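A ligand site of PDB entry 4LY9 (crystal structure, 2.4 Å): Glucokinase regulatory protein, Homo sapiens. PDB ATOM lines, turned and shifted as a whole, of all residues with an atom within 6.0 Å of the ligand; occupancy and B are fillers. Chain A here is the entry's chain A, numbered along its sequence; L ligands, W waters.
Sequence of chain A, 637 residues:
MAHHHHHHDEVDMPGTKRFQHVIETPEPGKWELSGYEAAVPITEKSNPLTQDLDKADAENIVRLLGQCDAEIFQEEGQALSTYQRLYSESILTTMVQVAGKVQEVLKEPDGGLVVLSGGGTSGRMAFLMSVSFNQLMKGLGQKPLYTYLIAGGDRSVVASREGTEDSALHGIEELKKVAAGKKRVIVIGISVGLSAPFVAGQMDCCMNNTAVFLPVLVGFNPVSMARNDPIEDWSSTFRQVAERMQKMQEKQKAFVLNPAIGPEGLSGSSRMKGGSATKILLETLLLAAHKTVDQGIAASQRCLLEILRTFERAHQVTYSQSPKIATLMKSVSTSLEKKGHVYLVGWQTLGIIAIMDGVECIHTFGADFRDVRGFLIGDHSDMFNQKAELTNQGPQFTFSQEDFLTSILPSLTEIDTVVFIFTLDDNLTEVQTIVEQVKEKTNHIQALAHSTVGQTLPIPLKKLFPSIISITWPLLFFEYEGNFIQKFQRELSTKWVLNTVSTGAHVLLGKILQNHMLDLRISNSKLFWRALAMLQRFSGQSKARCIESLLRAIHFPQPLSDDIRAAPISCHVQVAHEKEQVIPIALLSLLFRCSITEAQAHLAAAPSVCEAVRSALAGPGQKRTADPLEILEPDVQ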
ATOM      1  N   GLY A 119      15.071   0.083   0.025  1.00  0.00           N
ATOM      2  CA  GLY A 119      15.811   0.858  -0.975  1.00  0.00           C
ATOM      3  C   GLY A 119      16.425   2.061  -0.335  1.00  0.00           C
ATOM      4  O   GLY A 119      15.889   2.582   0.675  1.00  0.00           O
ATOM      5  N   GLY A 120      17.568   2.519  -0.896  1.00  0.00           N
ATOM      6  CA  GLY A 120      18.177   3.774  -0.483  1.00  0.00           C
ATOM      7  C   GLY A 120      18.488   3.788   1.016  1.00  0.00           C
ATOM      8  O   GLY A 120      19.041   2.789   1.579  1.00  0.00           O
ATOM      9  N   THR A 121      18.082   4.876   1.704  1.00  0.00           N
ATOM     10  CA  THR A 121      18.356   5.000   3.119  1.00  0.00           C
ATOM     11  C   THR A 121      17.691   3.962   3.906  1.00  0.00           C
ATOM     12  O   THR A 121      18.213   3.565   4.939  1.00  0.00           O
ATOM     13  CB  THR A 121      17.944   6.314   3.684  1.00  0.00           C
ATOM     14  OG1 THR A 121      18.537   7.357   2.923  1.00  0.00           O
ATOM     15  CG2 THR A 121      18.448   6.412   5.111  1.00  0.00           C
ATOM     16  N   SER A 122      16.536   3.483   3.464  1.00  0.00           N
ATOM     17  CA  SER A 122      15.968   2.347   4.178  1.00  0.00           C
ATOM     18  C   SER A 122      16.885   1.166   4.112  1.00  0.00           C
ATOM     19  O   SER A 122      16.935   0.385   5.069  1.00  0.00           O
ATOM     20  CB  SER A 122      14.609   1.946   3.644  1.00  0.00           C
ATOM     21  OG  SER A 122      13.766   3.059   3.853  1.00  0.00           O
ATOM     22  N   ARG A 124      20.242   1.254   3.747  1.00  0.00           N
ATOM     23  CA  ARG A 124      21.336   1.585   4.586  1.00  0.00           C
ATOM     24  C   ARG A 124      21.006   1.329   6.076  1.00  0.00           C
ATOM     25  O   ARG A 124      21.771   0.660   6.782  1.00  0.00           O
ATOM     26  CB  ARG A 124      21.680   3.033   4.394  1.00  0.00           C
ATOM     27  CG  ARG A 124      22.295   3.312   3.041  1.00  0.00           C
ATOM     28  CD  ARG A 124      22.815   4.739   2.991  1.00  0.00           C
ATOM     29  NE  ARG A 124      22.266   5.564   1.900  1.00  0.00           N
ATOM     30  CZ  ARG A 124      22.620   5.445   0.619  1.00  0.00           C
ATOM     31  NH1 ARG A 124      23.513   4.521   0.241  1.00  0.00           N
ATOM     32  NH2 ARG A 124      22.117   6.258  -0.294  1.00  0.00           N
ATOM     33  N   GLU A 162      19.871   5.786  -6.840  1.00  0.00           N
ATOM     34  CA  GLU A 162      18.442   6.000  -6.600  1.00  0.00           C
ATOM     35  C   GLU A 162      17.548   5.206  -7.585  1.00  0.00           C
ATOM     36  O   GLU A 162      16.402   4.917  -7.257  1.00  0.00           O
ATOM     37  CB  GLU A 162      18.141   7.478  -6.704  1.00  0.00           C
ATOM     38  CG  GLU A 162      18.660   8.266  -5.513  1.00  0.00           C
ATOM     39  CD  GLU A 162      17.758   8.052  -4.288  1.00  0.00           C
ATOM     40  OE1 GLU A 162      16.908   8.933  -4.008  1.00  0.00           O
ATOM     41  OE2 GLU A 162      17.911   6.985  -3.663  1.00  0.00           O
ATOM     42  N   GLU A 165      15.583   1.014  -6.939  1.00  0.00           N
ATOM     43  CA  GLU A 165      14.354   0.649  -6.205  1.00  0.00           C
ATOM     44  C   GLU A 165      13.050   0.275  -7.030  1.00  0.00           C
ATOM     45  O   GLU A 165      12.047  -0.173  -6.424  1.00  0.00           O
ATOM     46  CB  GLU A 165      14.073   1.747  -5.200  1.00  0.00           C
ATOM     47  CG  GLU A 165      13.569   3.082  -5.675  1.00  0.00           C
ATOM     48  CD  GLU A 165      12.973   3.945  -4.546  1.00  0.00           C
ATOM     49  OE1 GLU A 165      13.777   4.502  -3.789  1.00  0.00           O
ATOM     50  OE2 GLU A 165      11.713   4.140  -4.431  1.00  0.00           O
ATOM     51  N   ILE A 190      11.251  -2.425   4.614  1.00  0.00           N
ATOM     52  CA  ILE A 190      11.258  -1.061   5.080  1.00  0.00           C
ATOM     53  C   ILE A 190      11.076  -0.121   3.921  1.00  0.00           C
ATOM     54  O   ILE A 190      11.918  -0.050   3.069  1.00  0.00           O
ATOM     55  CB  ILE A 190      12.605  -0.732   5.789  1.00  0.00           C
ATOM     56  CG1 ILE A 190      12.904  -1.762   6.898  1.00  0.00           C
ATOM     57  CG2 ILE A 190      12.525   0.692   6.315  1.00  0.00           C
ATOM     58  CD1 ILE A 190      14.337  -1.751   7.453  1.00  0.00           C
ATOM     59  N   SER A 191       9.972   0.615   3.893  1.00  0.00           N
ATOM     60  CA  SER A 191       9.777   1.702   2.916  1.00  0.00           C
ATOM     61  C   SER A 191       8.992   2.826   3.556  1.00  0.00           C
ATOM     62  O   SER A 191       7.810   2.677   3.879  1.00  0.00           O
ATOM     63  CB  SER A 191       9.046   1.205   1.632  1.00  0.00           C
ATOM     64  OG  SER A 191       8.962   2.257   0.652  1.00  0.00           O
ATOM     65  N   VAL A 192       9.693   3.922   3.781  1.00  0.00           N
ATOM     66  CA  VAL A 192       9.231   4.980   4.545  1.00  0.00           C
ATOM     67  C   VAL A 192       7.945   5.485   3.970  1.00  0.00           C
ATOM     68  O   VAL A 192       7.012   5.795   4.685  1.00  0.00           O
ATOM     69  CB  VAL A 192      10.255   6.094   4.613  1.00  0.00           C
ATOM     70  CG1 VAL A 192       9.627   7.377   5.132  1.00  0.00           C
ATOM     71  CG2 VAL A 192      11.397   5.709   5.547  1.00  0.00           C
ATOM     72  N   GLY A 193       7.911   5.565   2.659  1.00  0.00           N
ATOM     73  CA  GLY A 193       6.743   6.068   1.967  1.00  0.00           C
ATOM     74  C   GLY A 193       5.750   5.010   1.627  1.00  0.00           C
ATOM     75  O   GLY A 193       4.726   5.331   1.019  1.00  0.00           O
ATOM     76  N   LEU A 194       5.990   3.769   2.065  1.00  0.00           N
ATOM     77  CA  LEU A 194       5.202   2.595   1.653  1.00  0.00           C
ATOM     78  C   LEU A 194       5.108   2.698   0.116  1.00  0.00           C
ATOM     79  O   LEU A 194       4.014   2.794  -0.484  1.00  0.00           O
ATOM     80  CB  LEU A 194       3.834   2.588   2.274  1.00  0.00           C
ATOM     81  CG  LEU A 194       3.732   2.464   3.788  1.00  0.00           C
ATOM     82  CD1 LEU A 194       2.299   2.109   4.187  1.00  0.00           C
ATOM     83  CD2 LEU A 194       4.673   1.378   4.294  1.00  0.00           C
ATOM     84  N   SER A 195       6.277   2.767  -0.479  1.00  0.00           N
ATOM     85  CA  SER A 195       6.457   3.206  -1.825  1.00  0.00           C
ATOM     86  C   SER A 195       7.287   2.266  -2.698  1.00  0.00           C
ATOM     87  O   SER A 195       6.960   2.173  -3.863  1.00  0.00           O
ATOM     88  CB  SER A 195       7.173   4.565  -1.802  1.00  0.00           C
ATOM     89  OG  SER A 195       7.775   4.810  -3.071  1.00  0.00           O
ATOM     90  N   ALA A 196       8.372   1.653  -2.184  1.00  0.00           N
ATOM     91  CA  ALA A 196       9.398   1.105  -3.085  1.00  0.00           C
ATOM     92  C   ALA A 196       8.976  -0.234  -3.744  1.00  0.00           C
ATOM     93  O   ALA A 196       8.582  -1.186  -3.048  1.00  0.00           O
ATOM     94  CB  ALA A 196      10.702   0.933  -2.347  1.00  0.00           C
ATOM     95  N   VAL A 199      10.362  -3.415  -2.300  1.00  0.00           N
ATOM     96  CA  VAL A 199       9.786  -4.036  -1.095  1.00  0.00           C
ATOM     97  C   VAL A 199       8.471  -4.670  -1.382  1.00  0.00           C
ATOM     98  O   VAL A 199       8.146  -5.756  -0.873  1.00  0.00           O
ATOM     99  CB  VAL A 199       9.633  -2.966  -0.012  1.00  0.00           C
ATOM    100  CG1 VAL A 199       8.896  -3.488   1.229  1.00  0.00           C
ATOM    101  CG2 VAL A 199      11.010  -2.422   0.380  1.00  0.00           C
ATOM    102  N   GLY A 268       9.825  15.432   1.549  1.00  0.00           N
ATOM    103  CA  GLY A 268      10.069  14.191   0.853  1.00  0.00           C
ATOM    104  C   GLY A 268      11.458  13.679   1.079  1.00  0.00           C
ATOM    105  O   GLY A 268      11.832  12.663   0.521  1.00  0.00           O
ATOM    106  N   SER A 269      12.236  14.320   1.948  1.00  0.00           N
ATOM    107  CA  SER A 269      13.586  13.834   2.192  1.00  0.00           C
ATOM    108  C   SER A 269      13.548  12.769   3.273  1.00  0.00           C
ATOM    109  O   SER A 269      14.035  12.981   4.392  1.00  0.00           O
ATOM    110  CB  SER A 269      14.541  14.988   2.537  1.00  0.00           C
ATOM    111  OG  SER A 269      15.870  14.467   2.621  1.00  0.00           O
ATOM    112  N   SER A 270      13.000  11.593   2.929  1.00  0.00           N
ATOM    113  CA  SER A 270      12.823  10.529   3.918  1.00  0.00           C
ATOM    114  C   SER A 270      14.157   9.961   4.478  1.00  0.00           C
ATOM    115  O   SER A 270      14.138   9.056   5.346  1.00  0.00           O
ATOM    116  CB  SER A 270      11.994   9.396   3.314  1.00  0.00           C
ATOM    117  OG  SER A 270      12.705   8.764   2.300  1.00  0.00           O
ATOM    118  N   ARG A 271      15.303  10.441   4.002  1.00  0.00           N
ATOM    119  CA  ARG A 271      16.554   9.980   4.629  1.00  0.00           C
ATOM    120  C   ARG A 271      16.620  10.467   6.079  1.00  0.00           C
ATOM    121  O   ARG A 271      17.263   9.840   6.903  1.00  0.00           O
ATOM    122  CB  ARG A 271      17.772  10.464   3.865  1.00  0.00           C
ATOM    123  CG  ARG A 271      17.995  11.967   3.941  1.00  0.00           C
ATOM    124  CD  ARG A 271      19.076  12.393   2.956  1.00  0.00           C
ATOM    125  NE  ARG A 271      19.637  13.719   3.302  1.00  0.00           N
ATOM    126  CZ  ARG A 271      20.832  13.902   3.876  1.00  0.00           C
ATOM    127  NH1 ARG A 271      21.632  12.867   4.151  1.00  0.00           N
ATOM    128  NH2 ARG A 271      21.226  15.123   4.192  1.00  0.00           N
ATOM    129  N   MET A 272      15.971  11.613   6.339  1.00  0.00           N
ATOM    130  CA  MET A 272      16.016  12.284   7.635  1.00  0.00           C
ATOM    131  C   MET A 272      15.127  11.623   8.716  1.00  0.00           C
ATOM    132  O   MET A 272      15.487  10.584   9.235  1.00  0.00           O
ATOM    133  CB  MET A 272      15.665  13.783   7.439  1.00  0.00           C
ATOM    134  CG  MET A 272      16.601  14.511   6.474  1.00  0.00           C
ATOM    135  SD  MET A 272      16.138  16.240   6.168  1.00  0.00           S
ATOM    136  CE  MET A 272      17.190  16.763   7.560  1.00  0.00           C
ATOM    137  N   GLU A 360      24.494  10.643   0.374  1.00  0.00           N
ATOM    138  CA  GLU A 360      23.098  11.013   0.170  1.00  0.00           C
ATOM    139  C   GLU A 360      22.981  12.414  -0.384  1.00  0.00           C
ATOM    140  O   GLU A 360      21.993  12.750  -1.069  1.00  0.00           O
ATOM    141  CB  GLU A 360      22.261  10.779   1.411  1.00  0.00           C
ATOM    142  CG  GLU A 360      22.114   9.271   1.670  1.00  0.00           C
ATOM    143  CD  GLU A 360      21.626   8.914   3.059  1.00  0.00           C
ATOM    144  OE1 GLU A 360      21.624   9.823   3.904  1.00  0.00           O
ATOM    145  OE2 GLU A 360      21.251   7.701   3.278  1.00  0.00           O
ATOM    146  N   HIS A 363      22.468  12.783  -4.604  1.00  0.00           N
ATOM    147  CA  HIS A 363      21.120  12.842  -5.163  1.00  0.00           C
ATOM    148  C   HIS A 363      20.290  13.894  -4.436  1.00  0.00           C
ATOM    149  O   HIS A 363      19.480  14.553  -5.043  1.00  0.00           O
ATOM    150  CB  HIS A 363      20.468  11.472  -5.159  1.00  0.00           C
ATOM    151  CG  HIS A 363      20.420  10.785  -3.816  1.00  0.00           C
ATOM    152  ND1 HIS A 363      21.138   9.647  -3.545  1.00  0.00           N
ATOM    153  CD2 HIS A 363      19.668  11.023  -2.715  1.00  0.00           C
ATOM    154  CE1 HIS A 363      20.868   9.222  -2.325  1.00  0.00           C
ATOM    155  NE2 HIS A 363      19.968  10.039  -1.797  1.00  0.00           N
ATOM    156  N   THR A 364      20.523  14.103  -3.147  1.00  0.00           N
ATOM    157  CA  THR A 364      19.613  14.964  -2.432  1.00  0.00           C
ATOM    158  C   THR A 364      19.812  16.370  -2.887  1.00  0.00           C
ATOM    159  O   THR A 364      18.829  17.094  -3.119  1.00  0.00           O
ATOM    160  CB  THR A 364      19.736  14.863  -0.911  1.00  0.00           C
ATOM    161  OG1 THR A 364      19.498  13.509  -0.516  1.00  0.00           O
ATOM    162  CG2 THR A 364      18.718  15.751  -0.261  1.00  0.00           C
ATOM    163  N   ASN A 524      14.168   7.970 -10.463  1.00  0.00           N
ATOM    164  CA  ASN A 524      13.206   6.881 -10.281  1.00  0.00           C
ATOM    165  C   ASN A 524      11.789   7.440 -10.408  1.00  0.00           C
ATOM    166  O   ASN A 524      11.596   8.668 -10.470  1.00  0.00           O
ATOM    167  CB  ASN A 524      13.439   6.095  -8.969  1.00  0.00           C
ATOM    168  CG  ASN A 524      13.323   6.955  -7.687  1.00  0.00           C
ATOM    169  OD1 ASN A 524      14.093   6.798  -6.722  1.00  0.00           O
ATOM    170  ND2 ASN A 524      12.364   7.786  -7.650  1.00  0.00           N
ATOM    171  N   LYS A 526       9.149   7.567  -8.306  1.00  0.00           N
ATOM    172  CA  LYS A 526       8.765   8.462  -7.219  1.00  0.00           C
ATOM    173  C   LYS A 526       9.254   9.940  -7.374  1.00  0.00           C
ATOM    174  O   LYS A 526       8.498  10.894  -7.185  1.00  0.00           O
ATOM    175  CB  LYS A 526       9.235   7.863  -5.911  1.00  0.00           C
ATOM    176  CG  LYS A 526       8.890   8.682  -4.687  1.00  0.00           C
ATOM    177  CD  LYS A 526       9.370   7.940  -3.450  1.00  0.00           C
ATOM    178  CE  LYS A 526      10.900   7.826  -3.360  1.00  0.00           C
ATOM    179  NZ  LYS A 526      11.184   7.050  -2.116  1.00  0.00           N
ATOM    180  N   ARG A 530       7.290  13.259  -7.768  1.00  0.00           N
ATOM    181  CA  ARG A 530       7.575  14.427  -6.928  1.00  0.00           C
ATOM    182  C   ARG A 530       7.821  15.637  -7.849  1.00  0.00           C
ATOM    183  O   ARG A 530       7.389  16.748  -7.571  1.00  0.00           O
ATOM    184  CB  ARG A 530       8.751  14.199  -5.986  1.00  0.00           C
ATOM    185  CG  ARG A 530       9.054  15.370  -5.023  1.00  0.00           C
ATOM    186  CD  ARG A 530      10.081  14.957  -3.945  1.00  0.00           C
ATOM    187  NE  ARG A 530       9.749  13.670  -3.270  1.00  0.00           N
ATOM    188  CZ  ARG A 530      10.625  12.807  -2.778  1.00  0.00           C
ATOM    189  NH1 ARG A 530      11.916  13.017  -2.906  1.00  0.00           N
ATOM    190  NH2 ARG A 530      10.238  11.686  -2.198  1.00  0.00           N
HETATM  191  C1  LIG L   1      15.338   9.884   0.518  1.00  0.00           C
HETATM  192  C2  LIG L   1      16.482   9.027   0.073  1.00  0.00           C
HETATM  193  C3  LIG L   1      15.939   7.946  -0.752  1.00  0.00           C
HETATM  194  C4  LIG L   1      15.010   6.994   0.004  1.00  0.00           C
HETATM  195  C5  LIG L   1      14.628   5.826  -0.904  1.00  0.00           C
HETATM  196  C6  LIG L   1      13.580   4.906  -0.313  1.00  0.00           C
HETATM  197  O1  LIG L   1      15.871  11.055   1.159  1.00  0.00           O
HETATM  198  O2  LIG L   1      17.297   9.860  -0.762  1.00  0.00           O
HETATM  199  O3  LIG L   1      17.031   7.200  -1.263  1.00  0.00           O
HETATM  200  O4  LIG L   1      15.638   6.493   1.198  1.00  0.00           O
HETATM  201  O5  LIG L   1      14.061   6.368  -2.117  1.00  0.00           O
HETATM  202  O6  LIG L   1      12.478   5.604   0.220  1.00  0.00           O
HETATM  203  P1  LIG L   1      11.395   4.730   0.880  1.00  0.00           P
HETATM  204  O7  LIG L   1      10.206   5.620   1.018  1.00  0.00           O
HETATM  205  O8  LIG L   1      12.003   4.169   2.190  1.00  0.00           O
HETATM  206  O9  LIG L   1      11.075   3.388   0.104  1.00  0.00           O
HETATM  207  O   HOH W   1      16.785  13.289   0.371  1.00  0.00           O
HETATM  208  O   HOH W   2      13.612   6.498   2.884  1.00  0.00           O
HETATM  209  O   HOH W   3      10.440   4.597  -2.298  1.00  0.00           O
HETATM  210  O   HOH W   4      12.462   0.946   0.464  1.00  0.00           O
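The side-chain hydroxyl of Ser 191 sits at hydrogen-bond distance from an oxygen (O9) of the ligand (2.5 Å). An oxygen (O5) of the ligand sits at hydrogen-bond distance from the side-chain carboxylate (OE1) of Glu 165, 2.5 Å away. An oxygen (O3) of the ligand lies within hydrogen-bond range of the side-chain carboxylate (OE2) of Glu 162, at 2.6 Å. The side-chain hydroxyl of Ser 122 is in hydrogen-bond range of an oxygen (O8) of the ligand (2.7 Å). The backbone NH (N) of Val 192 lies within hydrogen-bond range of an oxygen (O8) of the ligand, 2.8 Å away. O7 of the ligand is in hydrogen-bond range of N of Gly 193, at 2.8 Å. A ring nitrogen (NE2) of His 363 is in hydrogen-bond range of an oxygen (O2) of the ligand, 2.9 Å away. The side-chain amino group of Lys 526 lies within salt-bridge range of an oxygen (O7) of the ligand. An oxygen (O1) of the ligand lies within hydrogen-bond range of the backbone NH of Arg 271, at 3.0 Å. An oxygen (O4) of the ligand is in hydrogen-bond range of the backbone NH of Thr 121 (3.0 Å). The side-chain hydroxyl (OG1) of Thr 121 lies close to an oxygen (O4) of the ligand (3.5 Å). The backbone NH (N) of Ser 270 sits at hydrogen-bond distance from an oxygen (O1) of the ligand (3.4 Å).
Gly 119 touches the ligand. CA of Gly 120 touches O3 of the ligand (3.7 Å). CB of Ala 196 touches O9 of the ligand (3.5 Å). C of Ser 269 touches O1 of the ligand (3.6 Å). Hydrophobic or aromatic side chains that line the ligand: Val 192, Ala 196 and His 363.
Water W1 lies within hydrogen-bond range of an oxygen (O1) of the ligand, the side-chain hydroxyl (OG) of Ser 269 and the side-chain hydroxyl (OG1) of Thr 364. Water W2 bridges the side-chain hydroxyl of Ser 270 (2.5 Å) and an oxygen (O4) of the ligand (2.6 Å). Water W3 lies within hydrogen-bond range of the side-chain carboxylate (OE2) of Glu 165 (2.5 Å), the side-chain amino group (NZ) of Lys 526 (2.6 Å), an oxygen (O9) of the ligand (2.8 Å) and the side-chain hydroxyl (OG) of Ser 195 (2.8 Å). Water W4 lies within hydrogen-bond range of N of Gly 119 (2.8 Å), O9 of the ligand (2.8 Å) and O of Ile 190 (2.8 Å).
The side-chain hydroxyl (OG) of Ser 191 is in hydrogen-bond range of the backbone NH (N) of Ala 196 (3.0 Å). The backbone NH (N) of Ser 195 sits at hydrogen-bond distance from the side-chain hydroxyl (OG) of Ser 191, 3.0 Å away. The side-chain carboxylate (OE2) of Glu 165 is in salt-bridge range of the side-chain amino group (NZ) of Lys 526 (3.8 Å). O of Glu 162 lies close to OD1 of Asn 524 (3.0 Å). NE2 of His 363 sits close to O of Glu 360, 3.5 Å away. The backbone NH (N) of Lys 526 sits close to the side-chain amide nitrogen (ND2) of Asn 524 (3.3 Å). The guanidinium group (NH1) of Arg 271 lies within salt-bridge range of the side-chain carboxylate (OE1) of Glu 360. OE2 of Glu 360 is in hydrogen-bond range of OG1 of Thr 121 (2.8 Å).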
